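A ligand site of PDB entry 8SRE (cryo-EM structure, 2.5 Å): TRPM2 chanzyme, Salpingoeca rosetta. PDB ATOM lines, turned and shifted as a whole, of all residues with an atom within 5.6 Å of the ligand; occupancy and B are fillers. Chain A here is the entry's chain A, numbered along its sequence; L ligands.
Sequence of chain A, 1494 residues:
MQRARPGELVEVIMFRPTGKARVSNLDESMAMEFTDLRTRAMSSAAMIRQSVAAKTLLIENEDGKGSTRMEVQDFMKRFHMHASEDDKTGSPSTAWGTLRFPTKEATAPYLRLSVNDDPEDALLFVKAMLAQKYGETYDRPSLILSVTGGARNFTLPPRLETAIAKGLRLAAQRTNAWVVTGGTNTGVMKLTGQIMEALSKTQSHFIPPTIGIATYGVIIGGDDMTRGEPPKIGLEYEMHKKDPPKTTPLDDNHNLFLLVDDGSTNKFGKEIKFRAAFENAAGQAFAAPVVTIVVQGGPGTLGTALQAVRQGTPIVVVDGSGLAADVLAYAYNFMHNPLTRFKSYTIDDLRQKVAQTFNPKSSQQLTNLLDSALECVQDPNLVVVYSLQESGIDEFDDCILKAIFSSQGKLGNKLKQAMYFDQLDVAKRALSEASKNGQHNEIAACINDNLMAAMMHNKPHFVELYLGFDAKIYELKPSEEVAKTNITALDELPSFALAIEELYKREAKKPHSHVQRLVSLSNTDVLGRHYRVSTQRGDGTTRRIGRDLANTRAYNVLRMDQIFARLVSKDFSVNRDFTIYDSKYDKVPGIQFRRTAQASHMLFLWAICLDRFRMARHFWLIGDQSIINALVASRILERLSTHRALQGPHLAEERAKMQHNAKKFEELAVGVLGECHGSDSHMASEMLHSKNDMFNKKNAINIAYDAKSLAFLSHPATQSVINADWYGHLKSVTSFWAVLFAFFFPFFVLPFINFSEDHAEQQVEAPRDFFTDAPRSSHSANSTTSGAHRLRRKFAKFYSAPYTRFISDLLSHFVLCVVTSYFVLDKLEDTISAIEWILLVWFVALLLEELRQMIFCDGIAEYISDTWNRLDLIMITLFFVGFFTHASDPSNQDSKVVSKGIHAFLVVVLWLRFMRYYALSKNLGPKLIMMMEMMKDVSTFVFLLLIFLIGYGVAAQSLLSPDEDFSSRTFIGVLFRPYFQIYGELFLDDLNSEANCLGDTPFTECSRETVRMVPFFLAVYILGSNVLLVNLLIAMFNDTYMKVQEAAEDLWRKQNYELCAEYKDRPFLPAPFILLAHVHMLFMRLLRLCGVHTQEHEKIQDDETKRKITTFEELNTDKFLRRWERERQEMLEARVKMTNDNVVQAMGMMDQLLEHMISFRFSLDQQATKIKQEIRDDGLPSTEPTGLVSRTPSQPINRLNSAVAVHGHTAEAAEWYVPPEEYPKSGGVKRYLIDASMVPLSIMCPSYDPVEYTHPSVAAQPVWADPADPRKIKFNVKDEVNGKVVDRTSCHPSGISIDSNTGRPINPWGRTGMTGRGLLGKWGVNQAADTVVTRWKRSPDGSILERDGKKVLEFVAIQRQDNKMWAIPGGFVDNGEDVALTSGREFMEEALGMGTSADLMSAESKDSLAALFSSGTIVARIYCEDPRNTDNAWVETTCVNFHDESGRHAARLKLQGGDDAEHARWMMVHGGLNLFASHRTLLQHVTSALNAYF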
ATOM      1  N   VAL A 147     -21.691  18.687 -17.565  1.00  0.00           N
ATOM      2  CA  VAL A 147     -22.215  18.057 -18.775  1.00  0.00           C
ATOM      3  C   VAL A 147     -21.985  19.049 -19.903  1.00  0.00           C
ATOM      4  O   VAL A 147     -22.559  20.144 -19.898  1.00  0.00           O
ATOM      5  CB  VAL A 147     -23.687  17.660 -18.668  1.00  0.00           C
ATOM      6  CG1 VAL A 147     -24.068  16.799 -19.842  1.00  0.00           C
ATOM      7  CG2 VAL A 147     -23.905  16.883 -17.401  1.00  0.00           C
ATOM      8  N   THR A 148     -21.159  18.670 -20.863  1.00  0.00           N
ATOM      9  CA  THR A 148     -20.881  19.499 -22.017  1.00  0.00           C
ATOM     10  C   THR A 148     -21.126  18.726 -23.303  1.00  0.00           C
ATOM     11  O   THR A 148     -21.198  17.496 -23.309  1.00  0.00           O
ATOM     12  CB  THR A 148     -19.455  20.062 -22.017  1.00  0.00           C
ATOM     13  OG1 THR A 148     -19.241  20.831 -23.199  1.00  0.00           O
ATOM     14  CG2 THR A 148     -18.426  18.960 -21.979  1.00  0.00           C
ATOM     15  N   GLY A 149     -21.268  19.468 -24.388  1.00  0.00           N
ATOM     16  CA  GLY A 149     -21.430  18.866 -25.686  1.00  0.00           C
ATOM     17  C   GLY A 149     -22.141  19.775 -26.665  1.00  0.00           C
ATOM     18  O   GLY A 149     -21.978  20.997 -26.598  1.00  0.00           O
ATOM     19  N   GLY A 150     -22.858  19.146 -27.610  1.00  0.00           N
ATOM     20  CA  GLY A 150     -23.453  19.894 -28.716  1.00  0.00           C
ATOM     21  C   GLY A 150     -24.626  20.766 -28.311  1.00  0.00           C
ATOM     22  O   GLY A 150     -25.578  20.322 -27.680  1.00  0.00           O
ATOM     23  N   ALA A 151     -24.523  22.051 -28.635  1.00  0.00           N
ATOM     24  CA  ALA A 151     -25.659  22.938 -28.432  1.00  0.00           C
ATOM     25  C   ALA A 151     -26.735  22.843 -29.499  1.00  0.00           C
ATOM     26  O   ALA A 151     -27.869  22.533 -29.172  1.00  0.00           O
ATOM     27  CB  ALA A 151     -25.162  24.363 -28.312  1.00  0.00           C
ATOM     28  N   ARG A 152     -26.371  22.801 -30.783  1.00  0.00           N
ATOM     29  CA  ARG A 152     -27.389  22.767 -31.830  1.00  0.00           C
ATOM     30  C   ARG A 152     -27.358  21.508 -32.670  1.00  0.00           C
ATOM     31  O   ARG A 152     -28.414  20.937 -32.928  1.00  0.00           O
ATOM     32  CB  ARG A 152     -27.246  23.999 -32.735  1.00  0.00           C
ATOM     33  CG  ARG A 152     -27.853  25.247 -32.098  1.00  0.00           C
ATOM     34  CD  ARG A 152     -28.236  26.334 -33.102  1.00  0.00           C
ATOM     35  NE  ARG A 152     -28.728  27.553 -32.466  1.00  0.00           N
ATOM     36  CZ  ARG A 152     -29.971  27.753 -32.016  1.00  0.00           C
ATOM     37  NH1 ARG A 152     -30.906  26.823 -32.113  1.00  0.00           N
ATOM     38  NH2 ARG A 152     -30.268  28.912 -31.442  1.00  0.00           N
ATOM     39  N   ASN A 153     -26.167  21.060 -33.090  1.00  0.00           N
ATOM     40  CA  ASN A 153     -25.919  19.870 -33.904  1.00  0.00           C
ATOM     41  C   ASN A 153     -26.229  18.523 -33.209  1.00  0.00           C
ATOM     42  O   ASN A 153     -26.210  17.491 -33.884  1.00  0.00           O
ATOM     43  CB  ASN A 153     -24.454  19.858 -34.370  1.00  0.00           C
ATOM     44  CG  ASN A 153     -24.209  20.710 -35.622  1.00  0.00           C
ATOM     45  OD1 ASN A 153     -25.160  21.193 -36.233  1.00  0.00           O
ATOM     46  ND2 ASN A 153     -22.945  20.867 -36.014  1.00  0.00           N
ATOM     47  N   PHE A 154     -26.508  18.518 -31.907  1.00  0.00           N
ATOM     48  CA  PHE A 154     -26.852  17.386 -31.068  1.00  0.00           C
ATOM     49  C   PHE A 154     -28.133  16.898 -31.720  1.00  0.00           C
ATOM     50  O   PHE A 154     -29.105  17.643 -31.864  1.00  0.00           O
ATOM     51  CB  PHE A 154     -26.885  17.887 -29.620  1.00  0.00           C
ATOM     52  CG  PHE A 154     -27.066  16.820 -28.579  1.00  0.00           C
ATOM     53  CD1 PHE A 154     -25.947  16.155 -28.080  1.00  0.00           C
ATOM     54  CD2 PHE A 154     -28.331  16.593 -27.970  1.00  0.00           C
ATOM     55  CE1 PHE A 154     -26.070  15.185 -27.080  1.00  0.00           C
ATOM     56  CE2 PHE A 154     -28.475  15.618 -26.968  1.00  0.00           C
ATOM     57  CZ  PHE A 154     -27.339  14.931 -26.527  1.00  0.00           C
ATOM     58  N   GLY A 182     -24.201  24.325 -19.917  1.00  0.00           N
ATOM     59  CA  GLY A 182     -24.398  25.583 -20.583  1.00  0.00           C
ATOM     60  C   GLY A 182     -25.789  26.068 -20.215  1.00  0.00           C
ATOM     61  O   GLY A 182     -26.734  25.300 -20.075  1.00  0.00           O
ATOM     62  N   THR A 184     -27.996  27.643 -22.070  1.00  0.00           N
ATOM     63  CA  THR A 184     -29.002  27.805 -23.120  1.00  0.00           C
ATOM     64  C   THR A 184     -30.000  26.663 -23.264  1.00  0.00           C
ATOM     65  O   THR A 184     -29.779  25.542 -22.808  1.00  0.00           O
ATOM     66  CB  THR A 184     -28.270  27.982 -24.444  1.00  0.00           C
ATOM     67  OG1 THR A 184     -27.687  26.737 -24.816  1.00  0.00           O
ATOM     68  CG2 THR A 184     -27.111  28.990 -24.290  1.00  0.00           C
ATOM     69  N   THR A 186     -31.060  24.640 -25.624  1.00  0.00           N
ATOM     70  CA  THR A 186     -30.822  23.840 -26.813  1.00  0.00           C
ATOM     71  C   THR A 186     -29.965  22.644 -26.437  1.00  0.00           C
ATOM     72  O   THR A 186     -29.077  22.763 -25.595  1.00  0.00           O
ATOM     73  CB  THR A 186     -30.104  24.678 -27.902  1.00  0.00           C
ATOM     74  OG1 THR A 186     -29.016  25.422 -27.339  1.00  0.00           O
ATOM     75  CG2 THR A 186     -31.010  25.563 -28.816  1.00  0.00           C
ATOM     76  N   VAL A 188     -27.940  19.271 -25.470  1.00  0.00           N
ATOM     77  CA  VAL A 188     -27.548  18.468 -24.304  1.00  0.00           C
ATOM     78  C   VAL A 188     -27.828  19.219 -22.992  1.00  0.00           C
ATOM     79  O   VAL A 188     -28.103  18.585 -21.966  1.00  0.00           O
ATOM     80  CB  VAL A 188     -26.079  17.961 -24.483  1.00  0.00           C
ATOM     81  CG1 VAL A 188     -24.987  19.040 -24.349  1.00  0.00           C
ATOM     82  CG2 VAL A 188     -25.769  16.756 -23.582  1.00  0.00           C
ATOM     83  N   MET A 189     -27.752  20.566 -23.029  1.00  0.00           N
ATOM     84  CA  MET A 189     -28.085  21.446 -21.901  1.00  0.00           C
ATOM     85  C   MET A 189     -29.561  21.344 -21.554  1.00  0.00           C
ATOM     86  O   MET A 189     -29.931  21.271 -20.381  1.00  0.00           O
ATOM     87  CB  MET A 189     -27.727  22.876 -22.261  1.00  0.00           C
ATOM     88  CG  MET A 189     -26.315  23.108 -22.715  1.00  0.00           C
ATOM     89  SD  MET A 189     -26.280  24.593 -23.726  1.00  0.00           S
ATOM     90  CE  MET A 189     -24.586  24.591 -24.266  1.00  0.00           C
ATOM     91  N   THR A 248     -30.422  33.151 -29.161  1.00  0.00           N
ATOM     92  CA  THR A 248     -30.295  32.004 -28.277  1.00  0.00           C
ATOM     93  C   THR A 248     -30.892  32.248 -26.900  1.00  0.00           C
ATOM     94  O   THR A 248     -30.364  33.082 -26.151  1.00  0.00           O
ATOM     95  CB  THR A 248     -28.825  31.615 -28.164  1.00  0.00           C
ATOM     96  OG1 THR A 248     -28.312  31.327 -29.463  1.00  0.00           O
ATOM     97  CG2 THR A 248     -28.745  30.358 -27.413  1.00  0.00           C
ATOM     98  N   PHE A 268     -19.362  32.916 -29.662  1.00  0.00           N
ATOM     99  CA  PHE A 268     -19.463  31.804 -28.741  1.00  0.00           C
ATOM    100  C   PHE A 268     -18.089  31.355 -28.270  1.00  0.00           C
ATOM    101  O   PHE A 268     -17.054  31.726 -28.821  1.00  0.00           O
ATOM    102  CB  PHE A 268     -20.161  30.635 -29.430  1.00  0.00           C
ATOM    103  CG  PHE A 268     -21.591  30.908 -29.753  1.00  0.00           C
ATOM    104  CD1 PHE A 268     -22.577  30.824 -28.769  1.00  0.00           C
ATOM    105  CD2 PHE A 268     -21.949  31.220 -31.077  1.00  0.00           C
ATOM    106  CE1 PHE A 268     -23.932  31.040 -29.091  1.00  0.00           C
ATOM    107  CE2 PHE A 268     -23.296  31.459 -31.416  1.00  0.00           C
ATOM    108  CZ  PHE A 268     -24.285  31.374 -30.418  1.00  0.00           C
ATOM    109  N   GLY A 269     -18.108  30.533 -27.222  1.00  0.00           N
ATOM    110  CA  GLY A 269     -16.906  29.932 -26.683  1.00  0.00           C
ATOM    111  C   GLY A 269     -16.037  30.779 -25.795  1.00  0.00           C
ATOM    112  O   GLY A 269     -14.916  30.375 -25.473  1.00  0.00           O
ATOM    113  N   GLU A 271     -16.734  31.546 -22.668  1.00  0.00           N
ATOM    114  CA  GLU A 271     -16.952  31.197 -21.273  1.00  0.00           C
ATOM    115  C   GLU A 271     -16.286  29.899 -20.856  1.00  0.00           C
ATOM    116  O   GLU A 271     -16.349  29.588 -19.656  1.00  0.00           O
ATOM    117  CB  GLU A 271     -18.476  31.096 -21.038  1.00  0.00           C
ATOM    118  CG  GLU A 271     -19.221  29.731 -21.347  1.00  0.00           C
ATOM    119  CD  GLU A 271     -19.525  29.412 -22.813  1.00  0.00           C
ATOM    120  OE1 GLU A 271     -18.828  29.864 -23.745  1.00  0.00           O
ATOM    121  OE2 GLU A 271     -20.499  28.660 -23.033  1.00  0.00           O
ATOM    122  N   ILE A 272     -15.549  29.254 -21.774  1.00  0.00           N
ATOM    123  CA  ILE A 272     -14.955  27.914 -21.618  1.00  0.00           C
ATOM    124  C   ILE A 272     -13.888  27.840 -20.515  1.00  0.00           C
ATOM    125  O   ILE A 272     -13.932  26.938 -19.650  1.00  0.00           O
ATOM    126  CB  ILE A 272     -14.397  27.457 -22.986  1.00  0.00           C
ATOM    127  CG1 ILE A 272     -15.506  27.283 -24.042  1.00  0.00           C
ATOM    128  CG2 ILE A 272     -13.420  26.332 -22.926  1.00  0.00           C
ATOM    129  CD1 ILE A 272     -14.981  26.935 -25.440  1.00  0.00           C
ATOM    130  N   ARG A 275     -15.413  28.551 -17.074  1.00  0.00           N
ATOM    131  CA  ARG A 275     -16.234  27.395 -16.666  1.00  0.00           C
ATOM    132  C   ARG A 275     -15.381  26.272 -16.078  1.00  0.00           C
ATOM    133  O   ARG A 275     -15.722  25.755 -15.014  1.00  0.00           O
ATOM    134  CB  ARG A 275     -17.063  26.867 -17.839  1.00  0.00           C
ATOM    135  CG  ARG A 275     -17.988  25.717 -17.496  1.00  0.00           C
ATOM    136  CD  ARG A 275     -18.752  25.235 -18.701  1.00  0.00           C
ATOM    137  NE  ARG A 275     -19.258  23.881 -18.486  1.00  0.00           N
ATOM    138  CZ  ARG A 275     -20.117  23.273 -19.283  1.00  0.00           C
ATOM    139  NH1 ARG A 275     -20.595  23.868 -20.363  1.00  0.00           N
ATOM    140  NH2 ARG A 275     -20.499  22.039 -18.997  1.00  0.00           N
ATOM    141  N   GLY A 297     -20.891  16.914 -29.406  1.00  0.00           N
ATOM    142  CA  GLY A 297     -20.087  18.108 -29.354  1.00  0.00           C
ATOM    143  C   GLY A 297     -19.477  18.556 -30.668  1.00  0.00           C
ATOM    144  O   GLY A 297     -19.351  17.807 -31.634  1.00  0.00           O
ATOM    145  N   GLY A 298     -19.263  19.879 -30.709  1.00  0.00           N
ATOM    146  CA  GLY A 298     -18.623  20.618 -31.769  1.00  0.00           C
ATOM    147  C   GLY A 298     -17.219  21.059 -31.360  1.00  0.00           C
ATOM    148  O   GLY A 298     -16.593  20.420 -30.502  1.00  0.00           O
ATOM    149  N   PRO A 299     -16.658  22.097 -32.048  1.00  0.00           N
ATOM    150  CA  PRO A 299     -15.310  22.634 -31.690  1.00  0.00           C
ATOM    151  C   PRO A 299     -15.135  23.219 -30.282  1.00  0.00           C
ATOM    152  O   PRO A 299     -14.031  23.138 -29.711  1.00  0.00           O
ATOM    153  CB  PRO A 299     -15.094  23.729 -32.742  1.00  0.00           C
ATOM    154  CG  PRO A 299     -15.968  23.381 -33.858  1.00  0.00           C
ATOM    155  CD  PRO A 299     -17.178  22.737 -33.269  1.00  0.00           C
ATOM    156  N   GLY A 300     -16.182  23.858 -29.735  1.00  0.00           N
ATOM    157  CA  GLY A 300     -16.076  24.415 -28.389  1.00  0.00           C
ATOM    158  C   GLY A 300     -16.071  23.359 -27.300  1.00  0.00           C
ATOM    159  O   GLY A 300     -15.582  23.603 -26.197  1.00  0.00           O
ATOM    160  N   THR A 301     -16.687  22.190 -27.579  1.00  0.00           N
ATOM    161  CA  THR A 301     -16.656  21.054 -26.670  1.00  0.00           C
ATOM    162  C   THR A 301     -15.236  20.480 -26.555  1.00  0.00           C
ATOM    163  O   THR A 301     -14.809  20.049 -25.472  1.00  0.00           O
ATOM    164  CB  THR A 301     -17.657  20.049 -27.219  1.00  0.00           C
ATOM    165  OG1 THR A 301     -18.951  20.639 -27.131  1.00  0.00           O
ATOM    166  CG2 THR A 301     -17.725  18.753 -26.468  1.00  0.00           C
ATOM    167  N   LEU A 302     -14.506  20.507 -27.694  1.00  0.00           N
ATOM    168  CA  LEU A 302     -13.087  20.136 -27.787  1.00  0.00           C
ATOM    169  C   LEU A 302     -12.246  21.074 -26.944  1.00  0.00           C
ATOM    170  O   LEU A 302     -11.315  20.642 -26.251  1.00  0.00           O
ATOM    171  CB  LEU A 302     -12.623  20.129 -29.241  1.00  0.00           C
ATOM    172  CG  LEU A 302     -11.454  19.222 -29.607  1.00  0.00           C
ATOM    173  CD1 LEU A 302     -11.828  17.786 -29.331  1.00  0.00           C
ATOM    174  CD2 LEU A 302     -11.082  19.401 -31.058  1.00  0.00           C
ATOM    175  N   THR A 304     -13.482  22.862 -24.411  1.00  0.00           N
ATOM    176  CA  THR A 304     -13.965  22.587 -23.040  1.00  0.00           C
ATOM    177  C   THR A 304     -13.226  21.417 -22.402  1.00  0.00           C
ATOM    178  O   THR A 304     -12.766  21.517 -21.251  1.00  0.00           O
ATOM    179  CB  THR A 304     -15.479  22.368 -23.079  1.00  0.00           C
ATOM    180  OG1 THR A 304     -16.114  23.580 -23.501  1.00  0.00           O
ATOM    181  CG2 THR A 304     -16.059  21.994 -21.727  1.00  0.00           C
HETATM  182  N1  LIG L   1     -25.425  27.626 -26.922  1.00  0.00           N
HETATM  183  C1  LIG L   1     -26.112  27.755 -28.054  1.00  0.00           C
HETATM  184  N2  LIG L   1     -25.562  27.733 -29.267  1.00  0.00           N
HETATM  185  C2  LIG L   1     -24.230  27.584 -29.407  1.00  0.00           C
HETATM  186  C3  LIG L   1     -23.395  27.458 -28.215  1.00  0.00           C
HETATM  187  C4  LIG L   1     -24.085  27.486 -26.914  1.00  0.00           C
HETATM  188  N3  LIG L   1     -23.380  27.369 -25.769  1.00  0.00           N
HETATM  189  N4  LIG L   1     -22.136  27.330 -28.630  1.00  0.00           N
HETATM  190  C5  LIG L   1     -22.153  27.373 -29.982  1.00  0.00           C
HETATM  191  N5  LIG L   1     -23.399  27.530 -30.442  1.00  0.00           N
HETATM  192  C6  LIG L   1     -23.788  27.629 -31.857  1.00  0.00           C
HETATM  193  C7  LIG L   1     -22.510  27.672 -32.669  1.00  0.00           C
HETATM  194  O1  LIG L   1     -22.532  28.816 -33.524  1.00  0.00           O
HETATM  195  C8  LIG L   1     -22.515  26.438 -33.535  1.00  0.00           C
HETATM  196  O2  LIG L   1     -22.384  26.829 -34.899  1.00  0.00           O
HETATM  197  O3  LIG L   1     -24.505  26.460 -32.238  1.00  0.00           O
HETATM  198  C9  LIG L   1     -23.873  25.799 -33.326  1.00  0.00           C
HETATM  199  C10 LIG L   1     -23.712  24.320 -33.009  1.00  0.00           C
HETATM  200  O4  LIG L   1     -22.896  24.153 -31.861  1.00  0.00           O
HETATM  201  P1  LIG L   1     -22.342  22.682 -31.592  1.00  0.00           P
HETATM  202  O5  LIG L   1     -23.543  21.794 -31.462  1.00  0.00           O
HETATM  203  O6  LIG L   1     -21.338  22.409 -32.669  1.00  0.00           O
HETATM  204  O7  LIG L   1     -21.606  22.772 -30.166  1.00  0.00           O
HETATM  205  P2  LIG L   1     -20.240  23.571 -29.959  1.00  0.00           P
HETATM  206  O8  LIG L   1     -19.977  24.470 -31.129  1.00  0.00           O
HETATM  207  O9  LIG L   1     -19.179  22.646 -29.426  1.00  0.00           O
HETATM  208  O10 LIG L   1     -20.594  24.464 -28.689  1.00  0.00           O
HETATM  209  C11 LIG L   1     -21.261  23.784 -27.649  1.00  0.00           C
HETATM  210  O11 LIG L   1     -21.693  23.741 -25.313  1.00  0.00           O
HETATM  211  O12 LIG L   1     -21.098  22.771 -23.310  1.00  0.00           O
HETATM  212  C12 LIG L   1     -21.010  23.950 -24.094  1.00  0.00           C
HETATM  213  O13 LIG L   1     -19.108  25.347 -23.691  1.00  0.00           O
HETATM  214  C13 LIG L   1     -19.582  24.251 -24.477  1.00  0.00           C
HETATM  215  O14 LIG L   1     -19.251  26.025 -26.030  1.00  0.00           O
HETATM  216  C14 LIG L   1     -19.634  24.664 -25.928  1.00  0.00           C
HETATM  217  C15 LIG L   1     -21.082  24.511 -26.331  1.00  0.00           C
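The side-chain hydroxyl (OG1) of Thr 148 sits at hydrogen-bond distance from an oxygen (O12) of the ligand (2.7 Å).
The backbone NH (N) of Ala 151 sits at hydrogen-bond distance from an oxygen (O5) of the ligand (3.0 Å).
N of Gly 149 sits at hydrogen-bond distance from O12 of the ligand.
The backbone NH of Gly 298 lies within hydrogen-bond range of an oxygen (O9) of the ligand, 3.1 Å away.
N of Thr 301 lies within hydrogen-bond range of O9 of the ligand (3.1 Å).
An oxygen (O9) of the ligand is in hydrogen-bond range of the side-chain hydroxyl of Thr 301 (3.1 Å).
N of Arg 152 sits at hydrogen-bond distance from O5 of the ligand, at 3.1 Å.
N of Asn 153 is in hydrogen-bond range of O5 of the ligand.
NH1 of Arg 275 lies within hydrogen-bond range of O12 of the ligand (3.2 Å).
OG1 of Thr 184 is in hydrogen-bond range of N1 of the ligand (3.2 Å).
The backbone NH of Gly 300 lies within hydrogen-bond range of an oxygen (O9) of the ligand, 3.2 Å away.
O13 of the ligand lies within hydrogen-bond range of OG1 of Thr 304 (3.5 Å).
O of Gly 149 is in hydrogen-bond range of OG1 of Thr 301, 3.1 Å away.
The guanidinium group (NH2) of Arg 275 lies within hydrogen-bond range of the backbone carbonyl oxygen (O) of Val 147 (2.9 Å).
The side-chain sulfur (SD) of Met 189 sits at hydrogen-bond distance from the side-chain hydroxyl (OG1) of Thr 184 (2.8 Å).
The side-chain hydroxyl of Thr 186 lies within hydrogen-bond range of the side-chain hydroxyl of Thr 184.
O of Gly 300 is in hydrogen-bond range of OG1 of Thr 304, 2.7 Å away.
The backbone carbonyl oxygen (O) of Gly 150 sits at hydrogen-bond distance from the backbone NH (N) of Val 188, 3.4 Å away.
CA of Gly 150 touches O5 of the ligand (3.3 Å).
OG1 of Thr 186 touches C1 of the ligand, at 3.8 Å.
CE of Met 189 touches O11 of the ligand, 3.2 Å away.
Thr 248 touches the ligand.
Phe 268 touches the ligand (CE2 to O1, 3.5 Å).
OE2 of Glu 271 touches O13 of the ligand, at 3.7 Å.
Pro 299 touches the ligand.
Hydrophobic or aromatic side chains that line the ligand: Ala 151, Met 189, Phe 268 and Pro 299.
18 residues have an atom within 4 Å of the ligand: Thr 148, Gly 149, Gly 150, Ala 151, Arg 152, Asn 153, Thr 184, Thr 186, Met 189, Thr 248, Phe 268, Glu 271, Arg 275, Gly 298, Pro 299, Gly 300, Thr 301 and Thr 304.
The nearest printed residue that does not touch the ligand is Ile 272 (4.1 Å).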
